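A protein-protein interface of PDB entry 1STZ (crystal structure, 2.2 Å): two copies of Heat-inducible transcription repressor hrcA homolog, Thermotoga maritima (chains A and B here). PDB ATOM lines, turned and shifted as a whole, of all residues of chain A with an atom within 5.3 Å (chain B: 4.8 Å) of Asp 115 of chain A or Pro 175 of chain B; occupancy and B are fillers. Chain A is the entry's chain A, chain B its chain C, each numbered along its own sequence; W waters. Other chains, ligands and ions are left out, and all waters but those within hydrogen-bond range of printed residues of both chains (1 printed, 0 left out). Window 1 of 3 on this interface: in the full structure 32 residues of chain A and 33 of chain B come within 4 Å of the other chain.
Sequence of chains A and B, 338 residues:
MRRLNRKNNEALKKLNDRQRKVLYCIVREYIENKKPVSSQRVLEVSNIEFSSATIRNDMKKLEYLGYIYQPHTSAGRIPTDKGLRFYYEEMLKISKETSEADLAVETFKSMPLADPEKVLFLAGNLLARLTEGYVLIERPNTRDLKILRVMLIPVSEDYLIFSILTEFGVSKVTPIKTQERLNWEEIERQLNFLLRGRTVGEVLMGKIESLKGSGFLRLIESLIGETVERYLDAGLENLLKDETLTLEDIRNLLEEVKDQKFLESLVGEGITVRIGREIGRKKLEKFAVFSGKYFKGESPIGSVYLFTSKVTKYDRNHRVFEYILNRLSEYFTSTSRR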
ATOM      1  N   PRO A 112      13.601 -27.064   4.750  1.00  0.00           N
ATOM      2  CA  PRO A 112      14.700 -26.288   5.280  1.00  0.00           C
ATOM      3  C   PRO A 112      14.566 -26.031   6.778  1.00  0.00           C
ATOM      4  O   PRO A 112      15.145 -25.071   7.221  1.00  0.00           O
ATOM      5  CB  PRO A 112      14.613 -25.000   4.455  1.00  0.00           C
ATOM      6  CG  PRO A 112      13.172 -24.905   4.037  1.00  0.00           C
ATOM      7  CD  PRO A 112      12.479 -26.167   4.435  1.00  0.00           C
ATOM      8  N   LEU A 113      13.855 -26.857   7.541  1.00  0.00           N
ATOM      9  CA  LEU A 113      13.865 -26.715   9.004  1.00  0.00           C
ATOM     10  C   LEU A 113      15.267 -26.904   9.588  1.00  0.00           C
ATOM     11  O   LEU A 113      16.015 -27.748   9.131  1.00  0.00           O
ATOM     12  CB  LEU A 113      12.920 -27.710   9.669  1.00  0.00           C
ATOM     13  CG  LEU A 113      11.458 -27.638   9.250  1.00  0.00           C
ATOM     14  CD1 LEU A 113      10.713 -28.691  10.007  1.00  0.00           C
ATOM     15  CD2 LEU A 113      10.893 -26.242   9.487  1.00  0.00           C
ATOM     16  N   ALA A 114      15.604 -26.105  10.592  1.00  0.00           N
ATOM     17  CA  ALA A 114      16.913 -26.113  11.227  1.00  0.00           C
ATOM     18  C   ALA A 114      16.866 -26.450  12.735  1.00  0.00           C
ATOM     19  O   ALA A 114      17.889 -26.483  13.378  1.00  0.00           O
ATOM     20  CB  ALA A 114      17.579 -24.743  11.009  1.00  0.00           C
ATOM     21  N   ASP A 115      15.682 -26.681  13.294  1.00  0.00           N
ATOM     22  CA  ASP A 115      15.510 -27.019  14.710  1.00  0.00           C
ATOM     23  C   ASP A 115      15.402 -28.543  14.785  1.00  0.00           C
ATOM     24  O   ASP A 115      14.441 -29.121  14.294  1.00  0.00           O
ATOM     25  CB  ASP A 115      14.235 -26.353  15.270  1.00  0.00           C
ATOM     26  CG  ASP A 115      14.009 -26.603  16.784  1.00  0.00           C
ATOM     27  OD1 ASP A 115      14.658 -27.472  17.411  1.00  0.00           O
ATOM     28  OD2 ASP A 115      13.167 -25.939  17.432  1.00  0.00           O
ATOM     29  N   PRO A 116      16.385 -29.204  15.376  1.00  0.00           N
ATOM     30  CA  PRO A 116      16.341 -30.666  15.447  1.00  0.00           C
ATOM     31  C   PRO A 116      15.105 -31.186  16.202  1.00  0.00           C
ATOM     32  O   PRO A 116      14.626 -32.253  15.854  1.00  0.00           O
ATOM     33  CB  PRO A 116      17.653 -31.031  16.153  1.00  0.00           C
ATOM     34  CG  PRO A 116      18.084 -29.800  16.869  1.00  0.00           C
ATOM     35  CD  PRO A 116      17.596 -28.654  16.014  1.00  0.00           C
ATOM     36  N   GLU A 117      14.585 -30.427  17.161  1.00  0.00           N
ATOM     37  CA  GLU A 117      13.421 -30.837  17.937  1.00  0.00           C
ATOM     38  C   GLU A 117      12.178 -30.935  17.053  1.00  0.00           C
ATOM     39  O   GLU A 117      11.420 -31.904  17.147  1.00  0.00           O
ATOM     40  CB  GLU A 117      13.195 -29.883  19.116  1.00  0.00           C
ATOM     41  CG  GLU A 117      11.949 -30.146  19.958  1.00  0.00           C
ATOM     42  CD  GLU A 117      11.947 -31.512  20.649  1.00  0.00           C
ATOM     43  OE1 GLU A 117      10.840 -32.007  20.945  1.00  0.00           O
ATOM     44  OE2 GLU A 117      13.040 -32.091  20.887  1.00  0.00           O
ATOM     45  N   LYS A 118      11.988 -29.945  16.187  1.00  0.00           N
ATOM     46  CA  LYS A 118      10.875 -29.948  15.250  1.00  0.00           C
ATOM     47  C   LYS A 118      11.008 -31.091  14.205  1.00  0.00           C
ATOM     48  O   LYS A 118      10.001 -31.664  13.767  1.00  0.00           O
ATOM     49  CB  LYS A 118      10.766 -28.576  14.571  1.00  0.00           C
ATOM     50  CG  LYS A 118       9.642 -28.446  13.554  1.00  0.00           C
ATOM     51  CD  LYS A 118       8.263 -28.575  14.202  1.00  0.00           C
ATOM     52  CE  LYS A 118       7.151 -28.289  13.186  1.00  0.00           C
ATOM     53  NZ  LYS A 118       5.936 -27.722  13.840  1.00  0.00           N
ATOM     54  N   VAL A 119      12.234 -31.426  13.824  1.00  0.00           N
ATOM     55  CA  VAL A 119      12.449 -32.510  12.878  1.00  0.00           C
ATOM     56  C   VAL A 119      12.071 -33.849  13.530  1.00  0.00           C
ATOM     57  O   VAL A 119      11.417 -34.661  12.903  1.00  0.00           O
ATOM     58  CB  VAL A 119      13.895 -32.583  12.341  1.00  0.00           C
ATOM     59  CG1 VAL A 119      14.073 -33.833  11.510  1.00  0.00           C
ATOM     60  CG2 VAL A 119      14.219 -31.365  11.494  1.00  0.00           C
ATOM     61  N   PHE A 168      23.715 -29.799  15.769  1.00  0.00           N
ATOM     62  CA  PHE A 168      22.479 -30.245  15.116  1.00  0.00           C
ATOM     63  C   PHE A 168      21.516 -29.135  14.683  1.00  0.00           C
ATOM     64  O   PHE A 168      20.429 -29.425  14.193  1.00  0.00           O
ATOM     65  CB  PHE A 168      21.724 -31.191  16.059  1.00  0.00           C
ATOM     66  CG  PHE A 168      22.525 -32.375  16.490  1.00  0.00           C
ATOM     67  CD1 PHE A 168      22.646 -32.691  17.828  1.00  0.00           C
ATOM     68  CD2 PHE A 168      23.200 -33.150  15.551  1.00  0.00           C
ATOM     69  CE1 PHE A 168      23.391 -33.794  18.230  1.00  0.00           C
ATOM     70  CE2 PHE A 168      23.947 -34.251  15.942  1.00  0.00           C
ATOM     71  CZ  PHE A 168      24.038 -34.577  17.280  1.00  0.00           C
ATOM     72  N   VAL A 170      19.629 -25.047  15.299  1.00  0.00           N
ATOM     73  CA  VAL A 170      19.224 -23.962  16.198  1.00  0.00           C
ATOM     74  C   VAL A 170      18.191 -24.510  17.181  1.00  0.00           C
ATOM     75  O   VAL A 170      17.142 -25.022  16.777  1.00  0.00           O
ATOM     76  CB  VAL A 170      18.627 -22.812  15.382  1.00  0.00           C
ATOM     77  CG1 VAL A 170      18.274 -21.627  16.266  1.00  0.00           C
ATOM     78  CG2 VAL A 170      19.596 -22.393  14.268  1.00  0.00           C
ATOM     79  N   SER A 171      18.504 -24.454  18.467  1.00  0.00           N
ATOM     80  CA  SER A 171      17.629 -25.009  19.489  1.00  0.00           C
ATOM     81  C   SER A 171      17.219 -23.957  20.492  1.00  0.00           C
ATOM     82  O   SER A 171      17.800 -22.881  20.554  1.00  0.00           O
ATOM     83  CB  SER A 171      18.327 -26.150  20.224  1.00  0.00           C
ATOM     84  OG  SER A 171      18.966 -27.005  19.296  1.00  0.00           O
ATOM     85  N   LYS A 172      16.207 -24.307  21.273  1.00  0.00           N
ATOM     86  CA  LYS A 172      15.703 -23.503  22.376  1.00  0.00           C
ATOM     87  C   LYS A 172      15.195 -22.157  21.948  1.00  0.00           C
ATOM     88  O   LYS A 172      15.212 -21.231  22.736  1.00  0.00           O
ATOM     89  CB  LYS A 172      16.769 -23.299  23.443  1.00  0.00           C
ATOM     90  CG  LYS A 172      17.507 -24.540  23.827  1.00  0.00           C
ATOM     91  CD  LYS A 172      16.591 -25.525  24.440  1.00  0.00           C
ATOM     92  CE  LYS A 172      17.369 -26.565  25.182  1.00  0.00           C
ATOM     93  NZ  LYS A 172      16.436 -27.601  25.704  1.00  0.00           N
ATOM     94  N   VAL A 173      14.688 -22.062  20.728  1.00  0.00           N
ATOM     95  CA  VAL A 173      14.234 -20.789  20.204  1.00  0.00           C
ATOM     96  C   VAL A 173      13.058 -20.270  21.029  1.00  0.00           C
ATOM     97  O   VAL A 173      12.030 -20.931  21.163  1.00  0.00           O
ATOM     98  CB  VAL A 173      13.871 -20.860  18.704  1.00  0.00           C
ATOM     99  CG1 VAL A 173      13.738 -19.468  18.135  1.00  0.00           C
ATOM    100  CG2 VAL A 173      14.942 -21.582  17.941  1.00  0.00           C
ATOM    101  N   TYR A 331      19.049 -35.914   7.919  1.00  0.00           N
ATOM    102  CA  TYR A 331      18.984 -34.623   8.568  1.00  0.00           C
ATOM    103  C   TYR A 331      20.187 -34.441   9.530  1.00  0.00           C
ATOM    104  O   TYR A 331      20.908 -33.459   9.452  1.00  0.00           O
ATOM    105  CB  TYR A 331      17.655 -34.379   9.310  1.00  0.00           C
ATOM    106  CG  TYR A 331      17.717 -33.034  10.013  1.00  0.00           C
ATOM    107  CD1 TYR A 331      17.413 -31.850   9.338  1.00  0.00           C
ATOM    108  CD2 TYR A 331      18.189 -32.941  11.305  1.00  0.00           C
ATOM    109  CE1 TYR A 331      17.531 -30.611   9.975  1.00  0.00           C
ATOM    110  CE2 TYR A 331      18.327 -31.712  11.946  1.00  0.00           C
ATOM    111  CZ  TYR A 331      17.998 -30.550  11.279  1.00  0.00           C
ATOM    112  OH  TYR A 331      18.142 -29.341  11.949  1.00  0.00           O
ATOM    113  N   LEU B 160      18.699 -18.919   9.430  1.00  0.00           N
ATOM    114  CA  LEU B 160      17.959 -17.712   9.765  1.00  0.00           C
ATOM    115  C   LEU B 160      16.769 -18.061  10.613  1.00  0.00           C
ATOM    116  O   LEU B 160      16.427 -19.220  10.742  1.00  0.00           O
ATOM    117  CB  LEU B 160      17.568 -16.942   8.501  1.00  0.00           C
ATOM    118  CG  LEU B 160      16.504 -17.486   7.556  1.00  0.00           C
ATOM    119  CD1 LEU B 160      15.113 -17.196   8.090  1.00  0.00           C
ATOM    120  CD2 LEU B 160      16.686 -16.850   6.162  1.00  0.00           C
ATOM    121  N   ILE B 161      16.163 -17.068  11.242  1.00  0.00           N
ATOM    122  CA  ILE B 161      14.955 -17.300  11.999  1.00  0.00           C
ATOM    123  C   ILE B 161      13.804 -16.472  11.397  1.00  0.00           C
ATOM    124  O   ILE B 161      13.902 -15.269  11.213  1.00  0.00           O
ATOM    125  CB  ILE B 161      15.189 -16.966  13.499  1.00  0.00           C
ATOM    126  CG1 ILE B 161      16.149 -17.978  14.124  1.00  0.00           C
ATOM    127  CG2 ILE B 161      13.876 -16.978  14.266  1.00  0.00           C
ATOM    128  CD1 ILE B 161      16.896 -17.462  15.325  1.00  0.00           C
ATOM    129  N   VAL B 173       7.407 -19.173  15.087  1.00  0.00           N
ATOM    130  CA  VAL B 173       8.856 -19.052  15.139  1.00  0.00           C
ATOM    131  C   VAL B 173       9.506 -20.304  14.534  1.00  0.00           C
ATOM    132  O   VAL B 173       9.226 -21.421  14.974  1.00  0.00           O
ATOM    133  CB  VAL B 173       9.357 -18.852  16.577  1.00  0.00           C
ATOM    134  CG1 VAL B 173      10.812 -18.415  16.569  1.00  0.00           C
ATOM    135  CG2 VAL B 173       8.494 -17.813  17.308  1.00  0.00           C
ATOM    136  N   THR B 174      10.371 -20.113  13.539  1.00  0.00           N
ATOM    137  CA  THR B 174      10.910 -21.222  12.748  1.00  0.00           C
ATOM    138  C   THR B 174      12.342 -20.958  12.319  1.00  0.00           C
ATOM    139  O   THR B 174      12.592 -20.123  11.462  1.00  0.00           O
ATOM    140  CB  THR B 174      10.078 -21.447  11.468  1.00  0.00           C
ATOM    141  OG1 THR B 174       8.685 -21.549  11.777  1.00  0.00           O
ATOM    142  CG2 THR B 174      10.413 -22.795  10.841  1.00  0.00           C
ATOM    143  N   PRO B 175      13.292 -21.658  12.916  1.00  0.00           N
ATOM    144  CA  PRO B 175      14.657 -21.666  12.392  1.00  0.00           C
ATOM    145  C   PRO B 175      14.700 -22.379  11.028  1.00  0.00           C
ATOM    146  O   PRO B 175      14.084 -23.429  10.851  1.00  0.00           O
ATOM    147  CB  PRO B 175      15.446 -22.426  13.461  1.00  0.00           C
ATOM    148  CG  PRO B 175      14.554 -22.479  14.645  1.00  0.00           C
ATOM    149  CD  PRO B 175      13.156 -22.447  14.150  1.00  0.00           C
ATOM    150  N   ILE B 176      15.413 -21.788  10.077  1.00  0.00           N
ATOM    151  CA  ILE B 176      15.463 -22.288   8.702  1.00  0.00           C
ATOM    152  C   ILE B 176      16.916 -22.440   8.259  1.00  0.00           C
ATOM    153  O   ILE B 176      17.731 -21.562   8.475  1.00  0.00           O
ATOM    154  CB  ILE B 176      14.671 -21.330   7.778  1.00  0.00           C
ATOM    155  CG1 ILE B 176      13.188 -21.354   8.147  1.00  0.00           C
ATOM    156  CG2 ILE B 176      14.857 -21.664   6.291  1.00  0.00           C
ATOM    157  CD1 ILE B 176      12.359 -20.383   7.387  1.00  0.00           C
ATOM    158  N   LYS B 177      17.222 -23.582   7.668  1.00  0.00           N
ATOM    159  CA  LYS B 177      18.526 -23.901   7.125  1.00  0.00           C
ATOM    160  C   LYS B 177      18.560 -23.360   5.703  1.00  0.00           C
ATOM    161  O   LYS B 177      17.694 -23.675   4.891  1.00  0.00           O
ATOM    162  CB  LYS B 177      18.712 -25.425   7.120  1.00  0.00           C
ATOM    163  CG  LYS B 177      20.130 -25.907   6.922  1.00  0.00           C
ATOM    164  CD  LYS B 177      20.391 -27.266   7.596  1.00  0.00           C
ATOM    165  CE  LYS B 177      19.299 -28.289   7.319  1.00  0.00           C
ATOM    166  NZ  LYS B 177      19.808 -29.675   7.477  1.00  0.00           N
HETATM  167  O   HOH W   1      12.970 -25.409  12.391  1.00  0.00           O
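Val 173 of chain B touches its own counterpart, Val 173 of chain A.
Printed residues of chain A that touch a printed residue of chain B: Pro 112, Leu 113, Ala 114, Asp 115, Val 170, Val 173 and Tyr 331. Along chain A the printed residues that touch a printed residue of chain B span positions 112 to 331. Printed residues of chain B that touch a printed residue of chain A: Val 173, Thr 174, Pro 175, Ile 176 and Lys 177. Hydrophobic or aromatic side chains of chain B that line the printed part of chain A: Val 173, Pro 175 and Ile 176. Among the printed residues, 13 pairs touch across the chains. Among the printed residues, no Asp or Glu carboxylate lies within 4 Å of a Lys or Arg side-chain nitrogen of the other chain.
Among the printed residues, merely in contact across the chains: Pro 112 of chain A with Ile 176 of chain B (3.2 Å), Leu 113 of chain A with Thr 174 of chain B (3.7 Å), Leu 113 of chain A with Pro 175 of chain B (3.8 Å), Leu 113 of chain A with Lys 177 of chain B (3.8 Å), Ala 114 of chain A with Ile 176 of chain B (3.6 Å), Ala 114 of chain A with Lys 177 of chain B (3.6 Å), Asp 115 of chain A with Pro 175 of chain B (3.9 Å), Val 170 of chain A with Pro 175 of chain B (3.7 Å), Val 173 of chain A with Val 173 of chain B (3.5 Å), Val 173 of chain A with Pro 175 of chain B (3.4 Å) and Tyr 331 of chain A with Lys 177 of chain B (3.5 Å).
Asp 115 of chain A touches one residue of chain B. Of the printed residues of chain B, Leu 113 of chain A touches Thr 174, Pro 175 and Lys 177. Of the printed residues of chain A, Lys 177 of chain B touches Pro 112, Leu 113, Ala 114 and Tyr 331. Of the printed residues of chain A, Val 173 of chain B touches Val 173. Printed residues of chain B within 4 Å of Tyr 331 of chain A: Lys 177. Lys 172 of chain A touches none of the printed residues of chain B. The nearest printed residue of chain B that does not touch Asp 115 of chain A is Ile 176 of chain B (5.9 Å). The nearest printed residue of chain A that does not touch Val 173 of chain B is Asp 115 of chain A (6.5 Å).
Water W1 lies within hydrogen-bond range of the backbone carbonyl oxygen (O) of Pro 175 of chain B (2.7 Å), the backbone NH (N) of Asp 115 of chain A (3.1 Å) and the backbone NH (N) of Ala 114 of chain A (3.3 Å).
The backbone NH (N) of Val 170 of chain A sits at hydrogen-bond distance from the backbone carbonyl oxygen (O) of Ala 114 of chain A, 3.0 Å away. O of Ala 114 of chain A lies within hydrogen-bond range of OH of Tyr 331 of chain A. The side-chain carboxylate (OD1) of Asp 115 of chain A is in hydrogen-bond range of the backbone NH (N) of Glu 117 of chain A (3.0 Å). The side-chain hydroxyl (OH) of Tyr 331 of chain A sits at hydrogen-bond distance from the backbone carbonyl oxygen (O) of Phe 168 of chain A (3.2 Å). The backbone NH (N) of Ile 176 of chain B lies within hydrogen-bond range of the backbone carbonyl oxygen (O) of Leu 160 of chain B.
The backbone carbonyl oxygen of Pro 112 of chain A lies within hydrogen-bond range of the backbone NH of Lys 177 of chain B, 2.6 Å away. The backbone NH (N) of Ala 114 of chain A is in hydrogen-bond range of the backbone carbonyl oxygen (O) of Pro 175 of chain B.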
